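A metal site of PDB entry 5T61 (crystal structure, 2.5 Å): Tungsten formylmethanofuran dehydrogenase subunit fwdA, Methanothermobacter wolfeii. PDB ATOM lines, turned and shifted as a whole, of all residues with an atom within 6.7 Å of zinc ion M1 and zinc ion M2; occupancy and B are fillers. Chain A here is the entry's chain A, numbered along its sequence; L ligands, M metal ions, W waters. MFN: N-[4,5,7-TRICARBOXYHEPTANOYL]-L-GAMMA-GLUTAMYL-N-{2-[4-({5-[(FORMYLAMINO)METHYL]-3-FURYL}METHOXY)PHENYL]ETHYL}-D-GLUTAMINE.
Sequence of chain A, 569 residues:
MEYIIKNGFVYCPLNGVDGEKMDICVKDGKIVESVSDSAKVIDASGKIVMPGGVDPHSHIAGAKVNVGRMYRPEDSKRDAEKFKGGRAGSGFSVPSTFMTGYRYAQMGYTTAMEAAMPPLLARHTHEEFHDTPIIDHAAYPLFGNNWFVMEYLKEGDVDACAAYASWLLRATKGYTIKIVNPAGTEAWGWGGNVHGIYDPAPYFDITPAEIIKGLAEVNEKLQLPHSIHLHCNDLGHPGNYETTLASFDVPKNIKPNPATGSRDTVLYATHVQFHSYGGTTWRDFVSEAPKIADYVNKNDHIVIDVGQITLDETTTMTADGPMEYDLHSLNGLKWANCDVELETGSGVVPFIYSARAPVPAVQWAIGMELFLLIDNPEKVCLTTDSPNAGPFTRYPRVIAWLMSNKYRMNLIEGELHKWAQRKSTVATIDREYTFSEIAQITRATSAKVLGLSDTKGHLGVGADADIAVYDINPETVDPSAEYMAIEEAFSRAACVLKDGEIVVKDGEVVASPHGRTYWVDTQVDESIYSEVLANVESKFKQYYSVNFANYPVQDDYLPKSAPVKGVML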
ATOM      1  N   HIS A  57      18.071  28.483  -4.213  1.00  0.00           N
ATOM      2  CA  HIS A  57      18.074  27.062  -3.845  1.00  0.00           C
ATOM      3  C   HIS A  57      17.345  26.897  -2.512  1.00  0.00           C
ATOM      4  O   HIS A  57      17.902  27.204  -1.451  1.00  0.00           O
ATOM      5  CB  HIS A  57      19.497  26.530  -3.765  1.00  0.00           C
ATOM      6  CG  HIS A  57      19.563  25.031  -3.697  1.00  0.00           C
ATOM      7  ND1 HIS A  57      19.967  24.259  -4.757  1.00  0.00           N
ATOM      8  CD2 HIS A  57      19.222  24.167  -2.710  1.00  0.00           C
ATOM      9  CE1 HIS A  57      19.912  22.985  -4.426  1.00  0.00           C
ATOM     10  NE2 HIS A  57      19.464  22.898  -3.187  1.00  0.00           N
ATOM     11  N   SER A  58      16.116  26.390  -2.590  1.00  0.00           N
ATOM     12  CA  SER A  58      15.312  26.127  -1.407  1.00  0.00           C
ATOM     13  C   SER A  58      14.336  25.008  -1.736  1.00  0.00           C
ATOM     14  O   SER A  58      14.029  24.748  -2.907  1.00  0.00           O
ATOM     15  CB  SER A  58      14.570  27.391  -0.950  1.00  0.00           C
ATOM     16  OG  SER A  58      14.004  27.206   0.339  1.00  0.00           O
ATOM     17  N   HIS A  59      13.862  24.330  -0.697  1.00  0.00           N
ATOM     18  CA  HIS A  59      12.875  23.258  -0.818  1.00  0.00           C
ATOM     19  C   HIS A  59      11.590  23.726  -0.142  1.00  0.00           C
ATOM     20  O   HIS A  59      11.468  23.684   1.084  1.00  0.00           O
ATOM     21  CB  HIS A  59      13.438  21.977  -0.219  1.00  0.00           C
ATOM     22  CG  HIS A  59      14.645  21.465  -0.946  1.00  0.00           C
ATOM     23  ND1 HIS A  59      15.922  21.583  -0.457  1.00  0.00           N
ATOM     24  CD2 HIS A  59      14.756  20.823  -2.136  1.00  0.00           C
ATOM     25  CE1 HIS A  59      16.779  21.048  -1.318  1.00  0.00           C
ATOM     26  NE2 HIS A  59      16.093  20.580  -2.347  1.00  0.00           N
ATOM     27  N   ALA A 115      14.281  23.691  -5.669  1.00  0.00           N
ATOM     28  CA  ALA A 115      15.527  23.168  -6.220  1.00  0.00           C
ATOM     29  C   ALA A 115      15.469  21.703  -6.650  1.00  0.00           C
ATOM     30  O   ALA A 115      16.456  21.218  -7.220  1.00  0.00           O
ATOM     31  CB  ALA A 115      16.658  23.351  -5.212  1.00  0.00           C
ATOM     32  N   ALA A 116      14.378  20.975  -6.386  1.00  0.00           N
ATOM     33  CA  ALA A 116      14.354  19.553  -6.741  1.00  0.00           C
ATOM     34  C   ALA A 116      12.913  19.112  -6.948  1.00  0.00           C
ATOM     35  O   ALA A 116      12.201  18.819  -5.983  1.00  0.00           O
ATOM     36  CB  ALA A 116      15.038  18.722  -5.661  1.00  0.00           C
ATOM     37  N   KCX A 178      18.614  20.358 -13.019  1.00  0.00           N
ATOM     38  CA  KCX A 178      19.162  20.028 -11.670  1.00  0.00           C
ATOM     39  CB  KCX A 178      18.073  20.171 -10.611  1.00  0.00           C
ATOM     40  CG  KCX A 178      18.511  19.772  -9.196  1.00  0.00           C
ATOM     41  CD  KCX A 178      19.438  20.794  -8.543  1.00  0.00           C
ATOM     42  CE  KCX A 178      19.965  20.245  -7.220  1.00  0.00           C
ATOM     43  NZ  KCX A 178      18.963  20.164  -6.173  1.00  0.00           N
ATOM     44  C   KCX A 178      19.731  18.635 -11.700  1.00  0.00           C
ATOM     45  O   KCX A 178      19.181  17.738 -12.386  1.00  0.00           O
ATOM     46  CX  KCX A 178      19.267  19.888  -4.904  1.00  0.00           C
ATOM     47  OQ1 KCX A 178      20.390  19.599  -4.549  1.00  0.00           O
ATOM     48  OQ2 KCX A 178      18.312  19.918  -3.976  1.00  0.00           O
ATOM     49  N   ILE A 179      20.848  18.440 -11.006  1.00  0.00           N
ATOM     50  CA  ILE A 179      21.535  17.150 -10.951  1.00  0.00           C
ATOM     51  C   ILE A 179      21.886  16.847  -9.493  1.00  0.00           C
ATOM     52  O   ILE A 179      22.637  17.594  -8.872  1.00  0.00           O
ATOM     53  CB  ILE A 179      22.805  17.154 -11.819  1.00  0.00           C
ATOM     54  CG1 ILE A 179      22.497  17.576 -13.255  1.00  0.00           C
ATOM     55  CG2 ILE A 179      23.470  15.782 -11.778  1.00  0.00           C
ATOM     56  CD1 ILE A 179      23.745  17.887 -14.073  1.00  0.00           C
ATOM     57  N   VAL A 180      21.368  15.740  -8.962  1.00  0.00           N
ATOM     58  CA  VAL A 180      21.633  15.337  -7.585  1.00  0.00           C
ATOM     59  C   VAL A 180      22.211  13.928  -7.603  1.00  0.00           C
ATOM     60  O   VAL A 180      21.556  12.999  -8.088  1.00  0.00           O
ATOM     61  CB  VAL A 180      20.362  15.378  -6.712  1.00  0.00           C
ATOM     62  CG1 VAL A 180      20.664  14.827  -5.323  1.00  0.00           C
ATOM     63  CG2 VAL A 180      19.823  16.781  -6.631  1.00  0.00           C
ATOM     64  N   HIS A 231      24.515  19.007  -7.509  1.00  0.00           N
ATOM     65  CA  HIS A 231      24.644  18.434  -6.174  1.00  0.00           C
ATOM     66  C   HIS A 231      25.524  17.203  -6.329  1.00  0.00           C
ATOM     67  O   HIS A 231      25.130  16.225  -6.974  1.00  0.00           O
ATOM     68  CB  HIS A 231      23.238  18.131  -5.639  1.00  0.00           C
ATOM     69  CG  HIS A 231      23.189  17.242  -4.431  1.00  0.00           C
ATOM     70  ND1 HIS A 231      22.350  17.492  -3.372  1.00  0.00           N
ATOM     71  CD2 HIS A 231      23.793  16.057  -4.161  1.00  0.00           C
ATOM     72  CE1 HIS A 231      22.477  16.535  -2.465  1.00  0.00           C
ATOM     73  NE2 HIS A 231      23.342  15.653  -2.919  1.00  0.00           N
ATOM     74  N   LEU A 235      28.148  13.114  -1.067  1.00  0.00           N
ATOM     75  CA  LEU A 235      27.769  14.170  -0.130  1.00  0.00           C
ATOM     76  C   LEU A 235      27.920  13.720   1.312  1.00  0.00           C
ATOM     77  O   LEU A 235      27.532  12.604   1.676  1.00  0.00           O
ATOM     78  CB  LEU A 235      26.323  14.642  -0.370  1.00  0.00           C
ATOM     79  CG  LEU A 235      25.879  15.767   0.597  1.00  0.00           C
ATOM     80  CD1 LEU A 235      24.950  16.729  -0.113  1.00  0.00           C
ATOM     81  CD2 LEU A 235      25.163  15.257   1.891  1.00  0.00           C
ATOM     82  N   THR A 270      25.903  23.685  -5.604  1.00  0.00           N
ATOM     83  CA  THR A 270      25.043  24.078  -4.495  1.00  0.00           C
ATOM     84  C   THR A 270      25.470  23.384  -3.206  1.00  0.00           C
ATOM     85  O   THR A 270      26.091  22.322  -3.228  1.00  0.00           O
ATOM     86  CB  THR A 270      23.569  23.776  -4.808  1.00  0.00           C
ATOM     87  OG1 THR A 270      22.738  24.230  -3.735  1.00  0.00           O
ATOM     88  CG2 THR A 270      23.363  22.298  -5.046  1.00  0.00           C
ATOM     89  N   HIS A 271      25.110  24.019  -2.084  1.00  0.00           N
ATOM     90  CA  HIS A 271      25.469  23.641  -0.724  1.00  0.00           C
ATOM     91  C   HIS A 271      26.827  22.954  -0.652  1.00  0.00           C
ATOM     92  O   HIS A 271      26.941  21.820  -0.172  1.00  0.00           O
ATOM     93  CB  HIS A 271      24.391  22.754  -0.098  1.00  0.00           C
ATOM     94  CG  HIS A 271      23.929  21.629  -0.979  1.00  0.00           C
ATOM     95  ND1 HIS A 271      24.752  20.588  -1.350  1.00  0.00           N
ATOM     96  CD2 HIS A 271      22.717  21.379  -1.544  1.00  0.00           C
ATOM     97  CE1 HIS A 271      24.074  19.751  -2.125  1.00  0.00           C
ATOM     98  NE2 HIS A 271      22.849  20.206  -2.252  1.00  0.00           N
ATOM     99  N   HIS A 275      30.140  19.373   0.669  1.00  0.00           N
ATOM    100  CA  HIS A 275      31.053  18.712  -0.252  1.00  0.00           C
ATOM    101  C   HIS A 275      32.510  19.111   0.007  1.00  0.00           C
ATOM    102  O   HIS A 275      33.357  18.921  -0.863  1.00  0.00           O
ATOM    103  CB  HIS A 275      30.670  19.031  -1.699  1.00  0.00           C
ATOM    104  CG  HIS A 275      29.255  18.683  -2.043  1.00  0.00           C
ATOM    105  ND1 HIS A 275      28.827  17.391  -2.258  1.00  0.00           N
ATOM    106  CD2 HIS A 275      28.173  19.469  -2.232  1.00  0.00           C
ATOM    107  CE1 HIS A 275      27.543  17.390  -2.554  1.00  0.00           C
ATOM    108  NE2 HIS A 275      27.114  18.643  -2.540  1.00  0.00           N
ATOM    109  N   MET A 317      15.852  16.932   3.604  1.00  0.00           N
ATOM    110  CA  MET A 317      15.029  16.421   2.526  1.00  0.00           C
ATOM    111  C   MET A 317      15.770  16.639   1.214  1.00  0.00           C
ATOM    112  O   MET A 317      16.069  17.773   0.840  1.00  0.00           O
ATOM    113  CB  MET A 317      13.665  17.130   2.502  1.00  0.00           C
ATOM    114  CG  MET A 317      13.723  18.650   2.610  1.00  0.00           C
ATOM    115  SD  MET A 317      12.099  19.414   2.584  1.00  0.00           S
ATOM    116  CE  MET A 317      11.361  18.761   4.076  1.00  0.00           C
ATOM    117  N   THR A 318      16.058  15.540   0.503  1.00  0.00           N
ATOM    118  CA  THR A 318      16.921  15.610  -0.671  1.00  0.00           C
ATOM    119  C   THR A 318      16.447  14.552  -1.650  1.00  0.00           C
ATOM    120  O   THR A 318      15.753  13.600  -1.266  1.00  0.00           O
ATOM    121  CB  THR A 318      18.379  15.378  -0.306  1.00  0.00           C
ATOM    122  OG1 THR A 318      19.214  15.552  -1.468  1.00  0.00           O
ATOM    123  CG2 THR A 318      18.535  13.966   0.161  1.00  0.00           C
ATOM    124  N   ALA A 319      16.820  14.729  -2.911  1.00  0.00           N
ATOM    125  CA  ALA A 319      16.705  13.673  -3.904  1.00  0.00           C
ATOM    126  C   ALA A 319      17.836  12.650  -3.804  1.00  0.00           C
ATOM    127  O   ALA A 319      17.898  11.728  -4.614  1.00  0.00           O
ATOM    128  CB  ALA A 319      16.672  14.281  -5.309  1.00  0.00           C
ATOM    129  N   ASP A 320      18.722  12.813  -2.820  1.00  0.00           N
ATOM    130  CA  ASP A 320      19.826  11.898  -2.574  1.00  0.00           C
ATOM    131  C   ASP A 320      19.383  10.825  -1.591  1.00  0.00           C
ATOM    132  O   ASP A 320      19.777  10.787  -0.423  1.00  0.00           O
ATOM    133  CB  ASP A 320      21.031  12.691  -2.065  1.00  0.00           C
ATOM    134  CG  ASP A 320      22.349  11.973  -2.264  1.00  0.00           C
ATOM    135  OD1 ASP A 320      22.371  10.730  -2.286  1.00  0.00           O
ATOM    136  OD2 ASP A 320      23.359  12.690  -2.408  1.00  0.00           O
ATOM    137  N   ASP A 385      20.593  25.596   2.073  1.00  0.00           N
ATOM    138  CA  ASP A 385      19.896  24.490   1.406  1.00  0.00           C
ATOM    139  C   ASP A 385      18.574  24.196   2.111  1.00  0.00           C
ATOM    140  O   ASP A 385      18.233  23.054   2.414  1.00  0.00           O
ATOM    141  CB  ASP A 385      20.783  23.251   1.333  1.00  0.00           C
ATOM    142  CG  ASP A 385      20.176  22.160   0.476  1.00  0.00           C
ATOM    143  OD1 ASP A 385      19.282  22.462  -0.345  1.00  0.00           O
ATOM    144  OD2 ASP A 385      20.578  20.997   0.618  1.00  0.00           O
ATOM    145  N   SER A 386      17.839  25.270   2.383  1.00  0.00           N
ATOM    146  CA  SER A 386      16.702  25.247   3.288  1.00  0.00           C
ATOM    147  C   SER A 386      15.717  24.135   2.951  1.00  0.00           C
ATOM    148  O   SER A 386      15.305  23.995   1.802  1.00  0.00           O
ATOM    149  CB  SER A 386      15.978  26.594   3.261  1.00  0.00           C
ATOM    150  OG  SER A 386      14.921  26.616   4.193  1.00  0.00           O
ATOM    151  N   ASN A 388      17.708  21.975   4.754  1.00  0.00           N
ATOM    152  CA  ASN A 388      18.682  20.918   5.049  1.00  0.00           C
ATOM    153  C   ASN A 388      19.732  21.367   6.040  1.00  0.00           C
ATOM    154  O   ASN A 388      20.079  20.639   6.976  1.00  0.00           O
ATOM    155  CB  ASN A 388      19.372  20.431   3.771  1.00  0.00           C
ATOM    156  CG  ASN A 388      18.479  19.599   2.880  1.00  0.00           C
ATOM    157  OD1 ASN A 388      18.095  18.489   3.231  1.00  0.00           O
ATOM    158  ND2 ASN A 388      18.216  20.103   1.683  1.00  0.00           N
HETATM  159  C1  MFN L   1      21.929  18.261   0.474  1.00  0.00           C
HETATM  160  O1  MFN L   1      20.709  16.835   2.210  1.00  0.00           O
HETATM  161  C2  MFN L   1      21.726  17.635   1.859  1.00  0.00           C
HETATM  162  O2  MFN L   1      23.908  16.331   5.297  1.00  0.00           O
HETATM  163  C3  MFN L   1      22.604  17.837   2.958  1.00  0.00           C
HETATM  164  O3  MFN L   1      28.693  12.749  12.650  1.00  0.00           O
HETATM  165  C4  MFN L   1      22.036  17.108   4.001  1.00  0.00           C
HETATM  166  O4  MFN L   1      29.324   8.459  14.779  1.00  0.00           O
HETATM  167  C5  MFN L   1      20.882  16.499   3.516  1.00  0.00           C
HETATM  168  O5  MFN L   1      27.549   9.248  15.757  1.00  0.00           O
HETATM  169  C6  MFN L   1      25.736  14.878   8.939  1.00  0.00           C
HETATM  170  N3  MFN L   1      30.286  10.849  16.040  1.00  0.00           N
HETATM  171  C21 MFN L   1      31.434  11.750  16.045  1.00  0.00           C
HETATM  172  O6  MFN L   1      31.611  12.597  15.192  1.00  0.00           O
HETATM  173  C22 MFN L   1      32.426  11.550  17.177  1.00  0.00           C
HETATM  174  C14 MFN L   1      32.832  12.796  17.983  1.00  0.00           C
HETATM  175  C23 MFN L   1      33.398  12.351  19.320  1.00  0.00           C
HETATM  176  C24 MFN L   1      34.571  11.365  19.204  1.00  0.00           C
HETATM  177  O7  MFN L   1      35.701  11.712  19.642  1.00  0.00           O
HETATM  178  O8  MFN L   1      34.469  10.192  18.718  1.00  0.00           O
HETATM  179  N4  MFN L   1      33.907  13.490  20.010  1.00  0.00           N
HETATM  180  C25 MFN L   1      34.092  13.458  21.437  1.00  0.00           C
HETATM  181  O9  MFN L   1      33.807  12.451  22.049  1.00  0.00           O
HETATM  182  C26 MFN L   1      34.674  14.681  22.195  1.00  0.00           C
HETATM  183  C27 MFN L   1      36.153  14.330  22.638  1.00  0.00           C
HETATM  184  C28 MFN L   1      36.962  15.643  22.832  1.00  0.00           C
HETATM  185  C29 MFN L   1      36.494  16.315  24.085  1.00  0.00           C
HETATM  186  O10 MFN L   1      36.027  17.492  24.048  1.00  0.00           O
HETATM  187  O11 MFN L   1      36.581  15.710  25.198  1.00  0.00           O
HETATM  188  C19 MFN L   1      29.233  10.820  15.061  1.00  0.00           C
HETATM  189  C20 MFN L   1      28.661   9.442  15.196  1.00  0.00           C
HETATM  190  C16 MFN L   1      27.537  12.440  12.801  1.00  0.00           C
HETATM  191  C17 MFN L   1      27.052  11.851  14.166  1.00  0.00           C
HETATM  192  C18 MFN L   1      28.150  11.921  15.266  1.00  0.00           C
HETATM  193  N2  MFN L   1      26.584  12.598  11.699  1.00  0.00           N
HETATM  194  C15 MFN L   1      26.978  13.131  10.404  1.00  0.00           C
HETATM  195  C12 MFN L   1      26.522  14.630  10.206  1.00  0.00           C
HETATM  196  C11 MFN L   1      26.297  14.619   7.732  1.00  0.00           C
HETATM  197  C10 MFN L   1      25.686  15.022   6.549  1.00  0.00           C
HETATM  198  C7  MFN L   1      24.775  15.840   8.979  1.00  0.00           C
HETATM  199  C8  MFN L   1      24.061  16.190   7.820  1.00  0.00           C
HETATM  200  C9  MFN L   1      24.568  15.933   6.494  1.00  0.00           C
HETATM  201  C13 MFN L   1      22.620  16.982   5.443  1.00  0.00           C
HETATM  202  N1  MFN L   1      20.690  18.275  -0.262  1.00  0.00           N
HETATM  203  O12 MFN L   1      42.138  17.355  24.403  1.00  0.00           O
HETATM  204  C30 MFN L   1      40.943  17.743  24.472  1.00  0.00           C
HETATM  205  O13 MFN L   1      40.687  18.964  24.539  1.00  0.00           O
HETATM  206  C31 MFN L   1      39.840  16.733  24.467  1.00  0.00           C
HETATM  207  C32 MFN L   1      39.231  16.625  23.039  1.00  0.00           C
HETATM  208  C33 MFN L   1      38.451  15.331  22.915  1.00  0.00           C
HETATM  209  C34 MFN L   1      38.904  14.597  21.693  1.00  0.00           C
HETATM  210  O14 MFN L   1      39.263  13.389  21.780  1.00  0.00           O
HETATM  211  O15 MFN L   1      38.929  15.194  20.588  1.00  0.00           O
HETATM  212 ZN    ZN M   1      20.978  19.094  -2.726  1.00  0.00          ZN
HETATM  213 ZN    ZN M   2      18.800  21.234  -2.035  1.00  0.00          ZN
HETATM  214  O   HOH W   1      18.158  17.544  -3.392  1.00  0.00           O
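A nitrogen (N1) of the ligand is in salt-bridge range of the side-chain carboxylate (OD2) of Asp 385 (2.9 Å). OD1 of Asn 388 sits close to O1 of the ligand (3.3 Å). N1 of the ligand sits at hydrogen-bond distance from OG1 of Thr 318 (3.3 Å).
OQ2 of KCX 178 lies close to NE2 of His 59. NZ of KCX 178 lies within hydrogen-bond range of the backbone carbonyl oxygen of Ala 115 (2.9 Å). A ring nitrogen (ND1) of His 57 lies within hydrogen-bond range of the side-chain hydroxyl of Thr 270. A ring nitrogen (ND1) of His 59 lies close to the side-chain carboxylate (OD1) of Asp 385, 3.5 Å away. The side-chain carboxylate (OD2) of Asp 385 lies within hydrogen-bond range of the side-chain amide nitrogen (ND2) of Asn 388, 2.7 Å away. ND2 of Asn 388 lies close to ND1 of His 59 (3.5 Å). N of His 59 is in hydrogen-bond range of O of Ser 386. The backbone NH (N) of His 231 lies within hydrogen-bond range of the backbone carbonyl oxygen (O) of Ile 179, 2.7 Å away.
Within 4 Å of zinc ion M1: KCX 178, His 231, His 271 and Asp 385. The nearest printed residue that does not touch zinc ion M1 is His 57 (4.1 Å).
ND2 of Asn 388 touches zinc ion M2 (3.9 Å). Within 4 Å of zinc ion M2: His 57, His 59, KCX 178, His 271, Asp 385 and Asn 388. The nearest printed residue that does not touch zinc ion M2 is Ala 115 (4.4 Å).
Zinc ion M1 is bound by OQ1 of KCX 178 (2.0 Å), ND1 of His 231 (2.2 Å) and NE2 of His 271 (2.2 Å). Zinc ion M1 has three donor atoms within binding distance. Slightly farther from zinc ion M1 lies N1 of the ligand (2.6 Å).
Zinc ion M2 is bound by a ring nitrogen (NE2) of His 57 (2.1 Å), the side-chain carboxylate of Asp 385 (2.1 Å) and OQ2 of KCX 178 (2.4 Å). Zinc ion M2 has three donor atoms within binding distance. Slightly farther from zinc ion M2 lies a ring nitrogen (NE2) of His 59 (2.8 Å).
Water W1 bridges OG1 of Thr 318 (3.0 Å) and N of Ala 319 (3.2 Å).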
